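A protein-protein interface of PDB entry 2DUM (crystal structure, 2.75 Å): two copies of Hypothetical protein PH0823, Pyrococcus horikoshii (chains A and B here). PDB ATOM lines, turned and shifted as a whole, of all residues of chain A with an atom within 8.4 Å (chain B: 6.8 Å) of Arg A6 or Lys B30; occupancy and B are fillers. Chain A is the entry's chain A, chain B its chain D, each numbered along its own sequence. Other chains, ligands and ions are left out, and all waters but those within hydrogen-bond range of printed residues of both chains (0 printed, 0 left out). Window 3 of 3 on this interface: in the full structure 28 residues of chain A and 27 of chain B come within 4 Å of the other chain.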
ATOM      1  N   MET A   4      -1.868 -13.828 -16.108  1.00  0.00           N
ATOM      2  CA  MET A   4      -1.552 -13.724 -17.647  1.00  0.00           C
ATOM      3  C   MET A   4      -2.705 -13.429 -18.578  1.00  0.00           C
ATOM      4  O   MET A   4      -2.478 -12.866 -19.611  1.00  0.00           O
ATOM      5  CB  MET A   4      -0.883 -14.926 -18.405  1.00  0.00           C
ATOM      6  CG  MET A   4       0.545 -15.055 -18.126  1.00  0.00           C
ATOM      7  SD  MET A   4       1.802 -14.777 -19.397  1.00  0.00           S
ATOM      8  CE  MET A   4       1.012 -13.918 -20.759  1.00  0.00           C
ATOM      9  N   PHE A   5      -3.907 -13.897 -18.271  1.00  0.00           N
ATOM     10  CA  PHE A   5      -5.119 -13.477 -18.957  1.00  0.00           C
ATOM     11  C   PHE A   5      -5.777 -12.326 -18.176  1.00  0.00           C
ATOM     12  O   PHE A   5      -6.964 -12.030 -18.354  1.00  0.00           O
ATOM     13  CB  PHE A   5      -6.066 -14.697 -19.284  1.00  0.00           C
ATOM     14  CG  PHE A   5      -5.368 -15.754 -20.170  1.00  0.00           C
ATOM     15  CD1 PHE A   5      -5.502 -15.730 -21.574  1.00  0.00           C
ATOM     16  CD2 PHE A   5      -4.442 -16.695 -19.607  1.00  0.00           C
ATOM     17  CE1 PHE A   5      -4.831 -16.613 -22.405  1.00  0.00           C
ATOM     18  CE2 PHE A   5      -3.696 -17.625 -20.474  1.00  0.00           C
ATOM     19  CZ  PHE A   5      -3.920 -17.556 -21.870  1.00  0.00           C
ATOM     20  N   ARG A   6      -4.992 -11.637 -17.357  1.00  0.00           N
ATOM     21  CA  ARG A   6      -5.573 -10.587 -16.549  1.00  0.00           C
ATOM     22  C   ARG A   6      -6.048  -9.406 -17.378  1.00  0.00           C
ATOM     23  O   ARG A   6      -7.086  -8.800 -17.006  1.00  0.00           O
ATOM     24  CB  ARG A   6      -4.663 -10.119 -15.440  1.00  0.00           C
ATOM     25  CG  ARG A   6      -3.611  -9.384 -15.951  1.00  0.00           C
ATOM     26  CD  ARG A   6      -2.940  -8.577 -14.883  1.00  0.00           C
ATOM     27  NE  ARG A   6      -2.024  -9.359 -14.000  1.00  0.00           N
ATOM     28  CZ  ARG A   6      -1.606 -10.663 -14.062  1.00  0.00           C
ATOM     29  NH1 ARG A   6      -1.953 -11.604 -15.067  1.00  0.00           N
ATOM     30  NH2 ARG A   6      -0.768 -11.003 -13.030  1.00  0.00           N
ATOM     31  N   LYS A   7      -5.342  -9.081 -18.469  1.00  0.00           N
ATOM     32  CA  LYS A   7      -5.715  -7.988 -19.296  1.00  0.00           C
ATOM     33  C   LYS A   7      -5.208  -8.203 -20.734  1.00  0.00           C
ATOM     34  O   LYS A   7      -4.335  -7.554 -21.259  1.00  0.00           O
ATOM     35  CB  LYS A   7      -5.196  -6.710 -18.688  1.00  0.00           C
ATOM     36  CG  LYS A   7      -5.672  -5.426 -19.480  1.00  0.00           C
ATOM     37  CD  LYS A   7      -4.753  -4.247 -19.169  1.00  0.00           C
ATOM     38  CE  LYS A   7      -5.129  -3.558 -17.860  1.00  0.00           C
ATOM     39  NZ  LYS A   7      -5.807  -2.269 -18.312  1.00  0.00           N
ATOM     40  N   VAL A   8      -5.720  -9.170 -21.411  1.00  0.00           N
ATOM     41  CA  VAL A   8      -5.075  -9.416 -22.661  1.00  0.00           C
ATOM     42  C   VAL A   8      -5.494  -8.376 -23.663  1.00  0.00           C
ATOM     43  O   VAL A   8      -6.587  -7.784 -23.507  1.00  0.00           O
ATOM     44  CB  VAL A   8      -5.432 -10.824 -23.125  1.00  0.00           C
ATOM     45  CG1 VAL A   8      -5.402 -11.731 -21.926  1.00  0.00           C
ATOM     46  CG2 VAL A   8      -6.812 -10.848 -23.879  1.00  0.00           C
ATOM     47  N   LEU A   9      -4.655  -8.153 -24.687  1.00  0.00           N
ATOM     48  CA  LEU A   9      -5.025  -7.195 -25.743  1.00  0.00           C
ATOM     49  C   LEU A   9      -5.112  -8.015 -26.945  1.00  0.00           C
ATOM     50  O   LEU A   9      -4.392  -9.030 -27.084  1.00  0.00           O
ATOM     51  CB  LEU A   9      -3.886  -6.205 -25.974  1.00  0.00           C
ATOM     52  CG  LEU A   9      -3.702  -5.033 -26.961  1.00  0.00           C
ATOM     53  CD1 LEU A   9      -3.771  -5.476 -28.301  1.00  0.00           C
ATOM     54  CD2 LEU A   9      -4.742  -3.962 -26.786  1.00  0.00           C
ATOM     55  N   MET A  31     -10.149 -20.856 -19.770  1.00  0.00           N
ATOM     56  CA  MET A  31      -9.800 -20.139 -18.518  1.00  0.00           C
ATOM     57  C   MET A  31     -10.452 -18.768 -18.658  1.00  0.00           C
ATOM     58  O   MET A  31     -11.018 -18.413 -19.754  1.00  0.00           O
ATOM     59  CB  MET A  31      -8.273 -19.999 -18.299  1.00  0.00           C
ATOM     60  CG  MET A  31      -7.450 -21.292 -18.429  1.00  0.00           C
ATOM     61  SD  MET A  31      -5.831 -21.078 -17.832  1.00  0.00           S
ATOM     62  CE  MET A  31      -5.366 -19.621 -18.670  1.00  0.00           C
ATOM     63  N   GLU A  32     -10.429 -17.984 -17.592  1.00  0.00           N
ATOM     64  CA  GLU A  32     -11.206 -16.818 -17.724  1.00  0.00           C
ATOM     65  C   GLU A  32     -10.323 -15.575 -17.701  1.00  0.00           C
ATOM     66  O   GLU A  32      -9.543 -15.317 -16.768  1.00  0.00           O
ATOM     67  CB  GLU A  32     -12.319 -16.878 -16.719  1.00  0.00           C
ATOM     68  CG  GLU A  32     -12.036 -16.118 -15.463  1.00  0.00           C
ATOM     69  CD  GLU A  32     -13.322 -15.454 -14.895  1.00  0.00           C
ATOM     70  OE1 GLU A  32     -13.475 -15.520 -13.626  1.00  0.00           O
ATOM     71  OE2 GLU A  32     -14.156 -14.896 -15.719  1.00  0.00           O
ATOM     72  N   VAL A  33     -10.363 -14.880 -18.811  1.00  0.00           N
ATOM     73  CA  VAL A  33      -9.716 -13.584 -19.011  1.00  0.00           C
ATOM     74  C   VAL A  33     -10.248 -12.483 -18.001  1.00  0.00           C
ATOM     75  O   VAL A  33     -11.434 -12.529 -17.646  1.00  0.00           O
ATOM     76  CB  VAL A  33     -10.029 -13.205 -20.469  1.00  0.00           C
ATOM     77  CG1 VAL A  33      -9.218 -12.081 -20.910  1.00  0.00           C
ATOM     78  CG2 VAL A  33      -9.847 -14.438 -21.393  1.00  0.00           C
ATOM     79  N   GLY A  34      -9.392 -11.567 -17.494  1.00  0.00           N
ATOM     80  CA  GLY A  34      -9.795 -10.472 -16.579  1.00  0.00           C
ATOM     81  C   GLY A  34     -10.496  -9.463 -17.468  1.00  0.00           C
ATOM     82  O   GLY A  34     -11.719  -9.471 -17.566  1.00  0.00           O
ATOM     83  N   GLU A  35      -9.730  -8.640 -18.193  1.00  0.00           N
ATOM     84  CA  GLU A  35     -10.237  -7.676 -19.195  1.00  0.00           C
ATOM     85  C   GLU A  35      -9.622  -7.920 -20.559  1.00  0.00           C
ATOM     86  O   GLU A  35      -8.465  -8.193 -20.691  1.00  0.00           O
ATOM     87  CB  GLU A  35      -9.853  -6.296 -18.693  1.00  0.00           C
ATOM     88  CG  GLU A  35     -10.184  -4.974 -19.526  1.00  0.00           C
ATOM     89  CD  GLU A  35      -9.567  -3.693 -18.734  1.00  0.00           C
ATOM     90  OE1 GLU A  35      -9.387  -2.578 -19.312  1.00  0.00           O
ATOM     91  OE2 GLU A  35      -9.193  -3.817 -17.504  1.00  0.00           O
ATOM     92  N   VAL A  36     -10.379  -7.787 -21.606  1.00  0.00           N
ATOM     93  CA  VAL A  36      -9.742  -7.735 -22.950  1.00  0.00           C
ATOM     94  C   VAL A  36      -9.871  -6.336 -23.682  1.00  0.00           C
ATOM     95  O   VAL A  36     -10.941  -5.760 -23.773  1.00  0.00           O
ATOM     96  CB  VAL A  36     -10.201  -8.920 -23.855  1.00  0.00           C
ATOM     97  CG1 VAL A  36     -11.484  -9.340 -23.416  1.00  0.00           C
ATOM     98  CG2 VAL A  36     -10.239  -8.559 -25.370  1.00  0.00           C
ATOM     99  N   ILE A  37      -8.810  -5.778 -24.208  1.00  0.00           N
ATOM    100  CA  ILE A  37      -9.038  -4.577 -24.932  1.00  0.00           C
ATOM    101  C   ILE A  37      -9.027  -5.020 -26.375  1.00  0.00           C
ATOM    102  O   ILE A  37      -8.050  -5.557 -26.901  1.00  0.00           O
ATOM    103  CB  ILE A  37      -7.886  -3.648 -24.691  1.00  0.00           C
ATOM    104  CG1 ILE A  37      -7.749  -3.392 -23.232  1.00  0.00           C
ATOM    105  CG2 ILE A  37      -7.947  -2.367 -25.503  1.00  0.00           C
ATOM    106  CD1 ILE A  37      -6.276  -3.436 -22.845  1.00  0.00           C
ATOM    107  N   ALA A  93     -14.395 -13.494 -20.713  1.00  0.00           N
ATOM    108  CA  ALA A  93     -13.789 -12.352 -20.100  1.00  0.00           C
ATOM    109  C   ALA A  93     -14.675 -11.836 -18.935  1.00  0.00           C
ATOM    110  O   ALA A  93     -15.885 -11.749 -19.113  1.00  0.00           O
ATOM    111  CB  ALA A  93     -13.706 -11.291 -21.239  1.00  0.00           C
ATOM    112  N   LYS A  94     -14.160 -11.469 -17.770  1.00  0.00           N
ATOM    113  CA  LYS A  94     -14.991 -10.622 -16.947  1.00  0.00           C
ATOM    114  C   LYS A  94     -15.275  -9.202 -17.572  1.00  0.00           C
ATOM    115  O   LYS A  94     -16.341  -8.697 -17.274  1.00  0.00           O
ATOM    116  CB  LYS A  94     -14.442 -10.425 -15.569  1.00  0.00           C
ATOM    117  CG  LYS A  94     -13.479 -11.461 -15.115  1.00  0.00           C
ATOM    118  CD  LYS A  94     -13.861 -11.975 -13.729  1.00  0.00           C
ATOM    119  CE  LYS A  94     -13.284 -11.078 -12.657  1.00  0.00           C
ATOM    120  NZ  LYS A  94     -11.959 -10.310 -12.975  1.00  0.00           N
ATOM    121  N   ASN A  95     -14.397  -8.537 -18.373  1.00  0.00           N
ATOM    122  CA  ASN A  95     -14.678  -7.152 -18.920  1.00  0.00           C
ATOM    123  C   ASN A  95     -14.082  -6.905 -20.242  1.00  0.00           C
ATOM    124  O   ASN A  95     -13.084  -7.499 -20.622  1.00  0.00           O
ATOM    125  CB  ASN A  95     -14.171  -6.017 -18.076  1.00  0.00           C
ATOM    126  CG  ASN A  95     -14.767  -6.036 -16.732  1.00  0.00           C
ATOM    127  OD1 ASN A  95     -14.128  -6.479 -15.766  1.00  0.00           O
ATOM    128  ND2 ASN A  95     -16.052  -5.624 -16.630  1.00  0.00           N
ATOM    129  N   GLU A 116      -1.108   0.394 -21.767  1.00  0.00           N
ATOM    130  CA  GLU A 116      -2.060  -0.064 -20.797  1.00  0.00           C
ATOM    131  C   GLU A 116      -1.568  -1.143 -19.893  1.00  0.00           C
ATOM    132  O   GLU A 116      -2.397  -1.853 -19.289  1.00  0.00           O
ATOM    133  CB  GLU A 116      -3.295  -0.595 -21.445  1.00  0.00           C
ATOM    134  CG  GLU A 116      -4.408   0.330 -21.206  1.00  0.00           C
ATOM    135  CD  GLU A 116      -4.133   1.489 -22.026  1.00  0.00           C
ATOM    136  OE1 GLU A 116      -3.344   1.220 -22.978  1.00  0.00           O
ATOM    137  OE2 GLU A 116      -4.639   2.604 -21.698  1.00  0.00           O
ATOM    138  N   ASN A 117      -0.249  -1.257 -19.797  1.00  0.00           N
ATOM    139  CA  ASN A 117       0.369  -2.295 -19.074  1.00  0.00           C
ATOM    140  C   ASN A 117      -0.507  -3.558 -19.087  1.00  0.00           C
ATOM    141  O   ASN A 117      -1.156  -3.937 -18.090  1.00  0.00           O
ATOM    142  CB  ASN A 117       0.720  -1.836 -17.692  1.00  0.00           C
ATOM    143  CG  ASN A 117       1.686  -2.781 -17.052  1.00  0.00           C
ATOM    144  OD1 ASN A 117       1.657  -3.011 -15.837  1.00  0.00           O
ATOM    145  ND2 ASN A 117       2.517  -3.426 -17.885  1.00  0.00           N
ATOM    146  N   VAL A 118      -0.573  -4.176 -20.270  1.00  0.00           N
ATOM    147  CA  VAL A 118      -1.370  -5.378 -20.507  1.00  0.00           C
ATOM    148  C   VAL A 118      -0.546  -6.609 -20.148  1.00  0.00           C
ATOM    149  O   VAL A 118       0.680  -6.544 -20.179  1.00  0.00           O
ATOM    150  CB  VAL A 118      -1.852  -5.485 -21.977  1.00  0.00           C
ATOM    151  CG1 VAL A 118      -2.359  -4.243 -22.431  1.00  0.00           C
ATOM    152  CG2 VAL A 118      -0.764  -6.000 -22.940  1.00  0.00           C
ATOM    153  N   SER A 119      -1.234  -7.727 -19.854  1.00  0.00           N
ATOM    154  CA  SER A 119      -0.593  -8.964 -19.398  1.00  0.00           C
ATOM    155  C   SER A 119      -0.032  -9.729 -20.544  1.00  0.00           C
ATOM    156  O   SER A 119       1.010 -10.317 -20.374  1.00  0.00           O
ATOM    157  CB  SER A 119      -1.563  -9.867 -18.639  1.00  0.00           C
ATOM    158  OG  SER A 119      -2.715 -10.017 -19.419  1.00  0.00           O
ATOM    159  N   LEU A 120      -0.728  -9.693 -21.672  1.00  0.00           N
ATOM    160  CA  LEU A 120      -0.495 -10.507 -22.809  1.00  0.00           C
ATOM    161  C   LEU A 120      -0.929  -9.742 -24.013  1.00  0.00           C
ATOM    162  O   LEU A 120      -1.836  -8.908 -23.922  1.00  0.00           O
ATOM    163  CB  LEU A 120      -1.394 -11.717 -22.768  1.00  0.00           C
ATOM    164  CG  LEU A 120      -1.153 -12.752 -23.861  1.00  0.00           C
ATOM    165  CD1 LEU A 120       0.310 -13.084 -24.081  1.00  0.00           C
ATOM    166  CD2 LEU A 120      -1.754 -14.054 -23.509  1.00  0.00           C
ATOM    167  N   PHE B  25       8.155 -15.971 -16.330  1.00  0.00           N
ATOM    168  CA  PHE B  25       6.842 -16.499 -16.423  1.00  0.00           C
ATOM    169  C   PHE B  25       6.285 -16.540 -15.046  1.00  0.00           C
ATOM    170  O   PHE B  25       5.058 -16.436 -14.809  1.00  0.00           O
ATOM    171  CB  PHE B  25       6.866 -17.906 -16.993  1.00  0.00           C
ATOM    172  CG  PHE B  25       5.513 -18.429 -17.228  1.00  0.00           C
ATOM    173  CD1 PHE B  25       4.772 -18.979 -16.182  1.00  0.00           C
ATOM    174  CD2 PHE B  25       4.906 -18.254 -18.429  1.00  0.00           C
ATOM    175  CE1 PHE B  25       3.455 -19.418 -16.347  1.00  0.00           C
ATOM    176  CE2 PHE B  25       3.577 -18.702 -18.591  1.00  0.00           C
ATOM    177  CZ  PHE B  25       2.856 -19.300 -17.529  1.00  0.00           C
ATOM    178  N   GLU B  26       7.184 -16.714 -14.106  1.00  0.00           N
ATOM    179  CA  GLU B  26       6.694 -16.832 -12.769  1.00  0.00           C
ATOM    180  C   GLU B  26       6.268 -15.482 -12.263  1.00  0.00           C
ATOM    181  O   GLU B  26       5.360 -15.383 -11.388  1.00  0.00           O
ATOM    182  CB  GLU B  26       7.774 -17.331 -11.903  1.00  0.00           C
ATOM    183  CG  GLU B  26       7.516 -17.077 -10.502  1.00  0.00           C
ATOM    184  CD  GLU B  26       8.820 -16.994  -9.834  1.00  0.00           C
ATOM    185  OE1 GLU B  26       9.705 -16.310 -10.435  1.00  0.00           O
ATOM    186  OE2 GLU B  26       8.972 -17.648  -8.765  1.00  0.00           O
ATOM    187  N   LYS B  27       6.936 -14.458 -12.818  1.00  0.00           N
ATOM    188  CA  LYS B  27       6.672 -13.076 -12.478  1.00  0.00           C
ATOM    189  C   LYS B  27       5.409 -12.644 -13.102  1.00  0.00           C
ATOM    190  O   LYS B  27       4.654 -11.970 -12.459  1.00  0.00           O
ATOM    191  CB  LYS B  27       7.755 -12.187 -13.009  1.00  0.00           C
ATOM    192  CG  LYS B  27       9.046 -12.331 -12.293  1.00  0.00           C
ATOM    193  CD  LYS B  27       8.804 -12.154 -10.804  1.00  0.00           C
ATOM    194  CE  LYS B  27       9.065 -13.490 -10.120  1.00  0.00           C
ATOM    195  NZ  LYS B  27       8.718 -13.475  -8.665  1.00  0.00           N
ATOM    196  N   ARG B  28       5.154 -13.031 -14.344  1.00  0.00           N
ATOM    197  CA  ARG B  28       3.934 -12.611 -15.049  1.00  0.00           C
ATOM    198  C   ARG B  28       2.661 -13.455 -14.831  1.00  0.00           C
ATOM    199  O   ARG B  28       1.527 -12.996 -14.995  1.00  0.00           O
ATOM    200  CB  ARG B  28       4.178 -12.615 -16.564  1.00  0.00           C
ATOM    201  CG  ARG B  28       5.415 -11.970 -17.013  1.00  0.00           C
ATOM    202  CD  ARG B  28       5.051 -11.033 -18.124  1.00  0.00           C
ATOM    203  NE  ARG B  28       6.222 -10.268 -18.561  1.00  0.00           N
ATOM    204  CZ  ARG B  28       6.175  -8.977 -18.868  1.00  0.00           C
ATOM    205  NH1 ARG B  28       5.015  -8.311 -18.777  1.00  0.00           N
ATOM    206  NH2 ARG B  28       7.281  -8.354 -19.240  1.00  0.00           N
ATOM    207  N   ASN B  29       2.836 -14.731 -14.584  1.00  0.00           N
ATOM    208  CA  ASN B  29       1.674 -15.481 -14.497  1.00  0.00           C
ATOM    209  C   ASN B  29       1.212 -15.478 -13.067  1.00  0.00           C
ATOM    210  O   ASN B  29       2.026 -15.691 -12.142  1.00  0.00           O
ATOM    211  CB  ASN B  29       1.933 -16.869 -14.908  1.00  0.00           C
ATOM    212  CG  ASN B  29       0.699 -17.578 -15.027  1.00  0.00           C
ATOM    213  OD1 ASN B  29       0.520 -18.580 -14.377  1.00  0.00           O
ATOM    214  ND2 ASN B  29      -0.259 -16.994 -15.782  1.00  0.00           N
ATOM    215  N   LYS B  30      -0.082 -15.206 -12.857  1.00  0.00           N
ATOM    216  CA  LYS B  30      -0.684 -15.557 -11.558  1.00  0.00           C
ATOM    217  C   LYS B  30      -1.699 -16.680 -11.760  1.00  0.00           C
ATOM    218  O   LYS B  30      -2.199 -17.256 -10.812  1.00  0.00           O
ATOM    219  CB  LYS B  30      -1.252 -14.332 -10.791  1.00  0.00           C
ATOM    220  CG  LYS B  30      -0.189 -13.117 -10.382  1.00  0.00           C
ATOM    221  CD  LYS B  30       0.759 -13.253  -9.040  1.00  0.00           C
ATOM    222  CE  LYS B  30       2.383 -12.987  -9.281  1.00  0.00           C
ATOM    223  NZ  LYS B  30       3.181 -13.821 -10.331  1.00  0.00           N
ATOM    224  N   MET B  31      -1.976 -17.010 -13.004  1.00  0.00           N
ATOM    225  CA  MET B  31      -2.952 -18.027 -13.345  1.00  0.00           C
ATOM    226  C   MET B  31      -2.423 -19.439 -13.152  1.00  0.00           C
ATOM    227  O   MET B  31      -1.249 -19.672 -13.253  1.00  0.00           O
ATOM    228  CB  MET B  31      -3.497 -17.797 -14.759  1.00  0.00           C
ATOM    229  CG  MET B  31      -4.232 -16.447 -14.901  1.00  0.00           C
ATOM    230  SD  MET B  31      -5.074 -16.733 -16.375  1.00  0.00           S
ATOM    231  CE  MET B  31      -6.743 -16.799 -15.640  1.00  0.00           C
ATOM    232  N   GLU B  32      -3.317 -20.362 -12.812  1.00  0.00           N
ATOM    233  CA  GLU B  32      -2.939 -21.703 -12.526  1.00  0.00           C
ATOM    234  C   GLU B  32      -2.753 -22.491 -13.855  1.00  0.00           C
ATOM    235  O   GLU B  32      -3.537 -22.344 -14.815  1.00  0.00           O
ATOM    236  CB  GLU B  32      -4.007 -22.337 -11.669  1.00  0.00           C
ATOM    237  CG  GLU B  32      -3.658 -23.809 -11.369  1.00  0.00           C
ATOM    238  CD  GLU B  32      -4.881 -24.815 -11.091  1.00  0.00           C
ATOM    239  OE1 GLU B  32      -5.193 -25.036  -9.847  1.00  0.00           O
ATOM    240  OE2 GLU B  32      -5.437 -25.430 -12.101  1.00  0.00           O
ATOM    241  N   ARG B  92       2.026 -22.184 -12.572  1.00  0.00           N
ATOM    242  CA  ARG B  92       1.332 -22.574 -11.375  1.00  0.00           C
ATOM    243  C   ARG B  92       0.714 -23.907 -11.617  1.00  0.00           C
ATOM    244  O   ARG B  92      -0.468 -24.060 -11.375  1.00  0.00           O
ATOM    245  CB  ARG B  92       0.407 -21.476 -10.864  1.00  0.00           C
ATOM    246  CG  ARG B  92       1.207 -20.352 -10.274  1.00  0.00           C
ATOM    247  CD  ARG B  92       1.118 -19.115 -11.160  1.00  0.00           C
ATOM    248  NE  ARG B  92       2.182 -18.164 -10.841  1.00  0.00           N
ATOM    249  CZ  ARG B  92       2.194 -17.393  -9.758  1.00  0.00           C
ATOM    250  NH1 ARG B  92       1.154 -17.454  -8.895  1.00  0.00           N
ATOM    251  NH2 ARG B  92       3.238 -16.567  -9.552  1.00  0.00           N
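Of chain B, only Arg B28 (3.6 Å) and Lys B30 (3.4 Å) come within 4 Å of Arg A6.
Lys B30 touches just these residues of chain A: Met A4 (3.96 Å) and Arg A6 (3.4 Å).
Asn B29 touches one residue of chain A.
Printed residues of chain A within 4 Å of Glu B32: Met A31.
Of the printed residues of chain B, Met A4 touches Arg B28 (3.7 Å), Asn B29 (3.1 Å), Lys B30 (3.96 Å) and Met B31 (3.7 Å).
Lys A94 touches none of the printed residues of chain B.
Asn A95 touches none of the printed residues of chain B.
The nearest residue of chain A that does not touch Lys B30 is Phe A5 (6.8 Å).
The nearest printed residue of chain B that does not touch Met A31 is Asn B29 (6.4 Å).
Among the printed residues, pairs that only touch across the chains: Met A4 with Asn B29 (3.1 Å), Glu A32 with Met B31 (3.4 Å), Arg A6 with Lys B30 (3.4 Å), Arg A6 with Arg B28 (3.6 Å), Met A4 with Arg B28 (3.7 Å), Met A31 with Met B31 (3.7 Å), Met A4 with Met B31 (3.7 Å), Met A4 with Lys B30 (3.96 Å) and Met A31 with Glu B32 (3.996 Å).
Met A31 touches its own counterpart, Met B31.
Met A31 touches Glu B32, and with the chains exchanged Glu A32 touches Met B31.
2 positions are printed for both chains.
Of the 10 pairs that touch across the chains among the printed residues, 3 have their exchanged pair printed and touching as well.
Hydrophobic or aromatic side chains of chain B within 4 Å of the printed part of chain A: Met B31.
Along chain B the printed residues that touch a printed residue of chain A span positions 28 to 32.
Among the printed residues, no Asp or Glu carboxylate lies within 4 Å of a Lys or Arg side-chain nitrogen of the other chain.
The backbone carbonyl oxygen (O) of Arg A6 sits at hydrogen-bond distance from the backbone NH (N) of Glu A35 (2.9 Å).
The backbone NH of Gly A34 sits at hydrogen-bond distance from the backbone carbonyl oxygen of Phe A5 (2.6 Å).
O of Lys B27 sits at hydrogen-bond distance from NZ of Lys B30 (3.2 Å).
The backbone NH of Met B31 sits at hydrogen-bond distance from the side-chain amide oxygen of Asn B29.
NH1 of Arg A6 lies close to N of Met A4.
The backbone carbonyl oxygen (O) of Met A4 sits at hydrogen-bond distance from the side-chain hydroxyl (OG) of Ser A119.
SD of Met B31 sits close to N of Phe A5 (3.6 Å).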
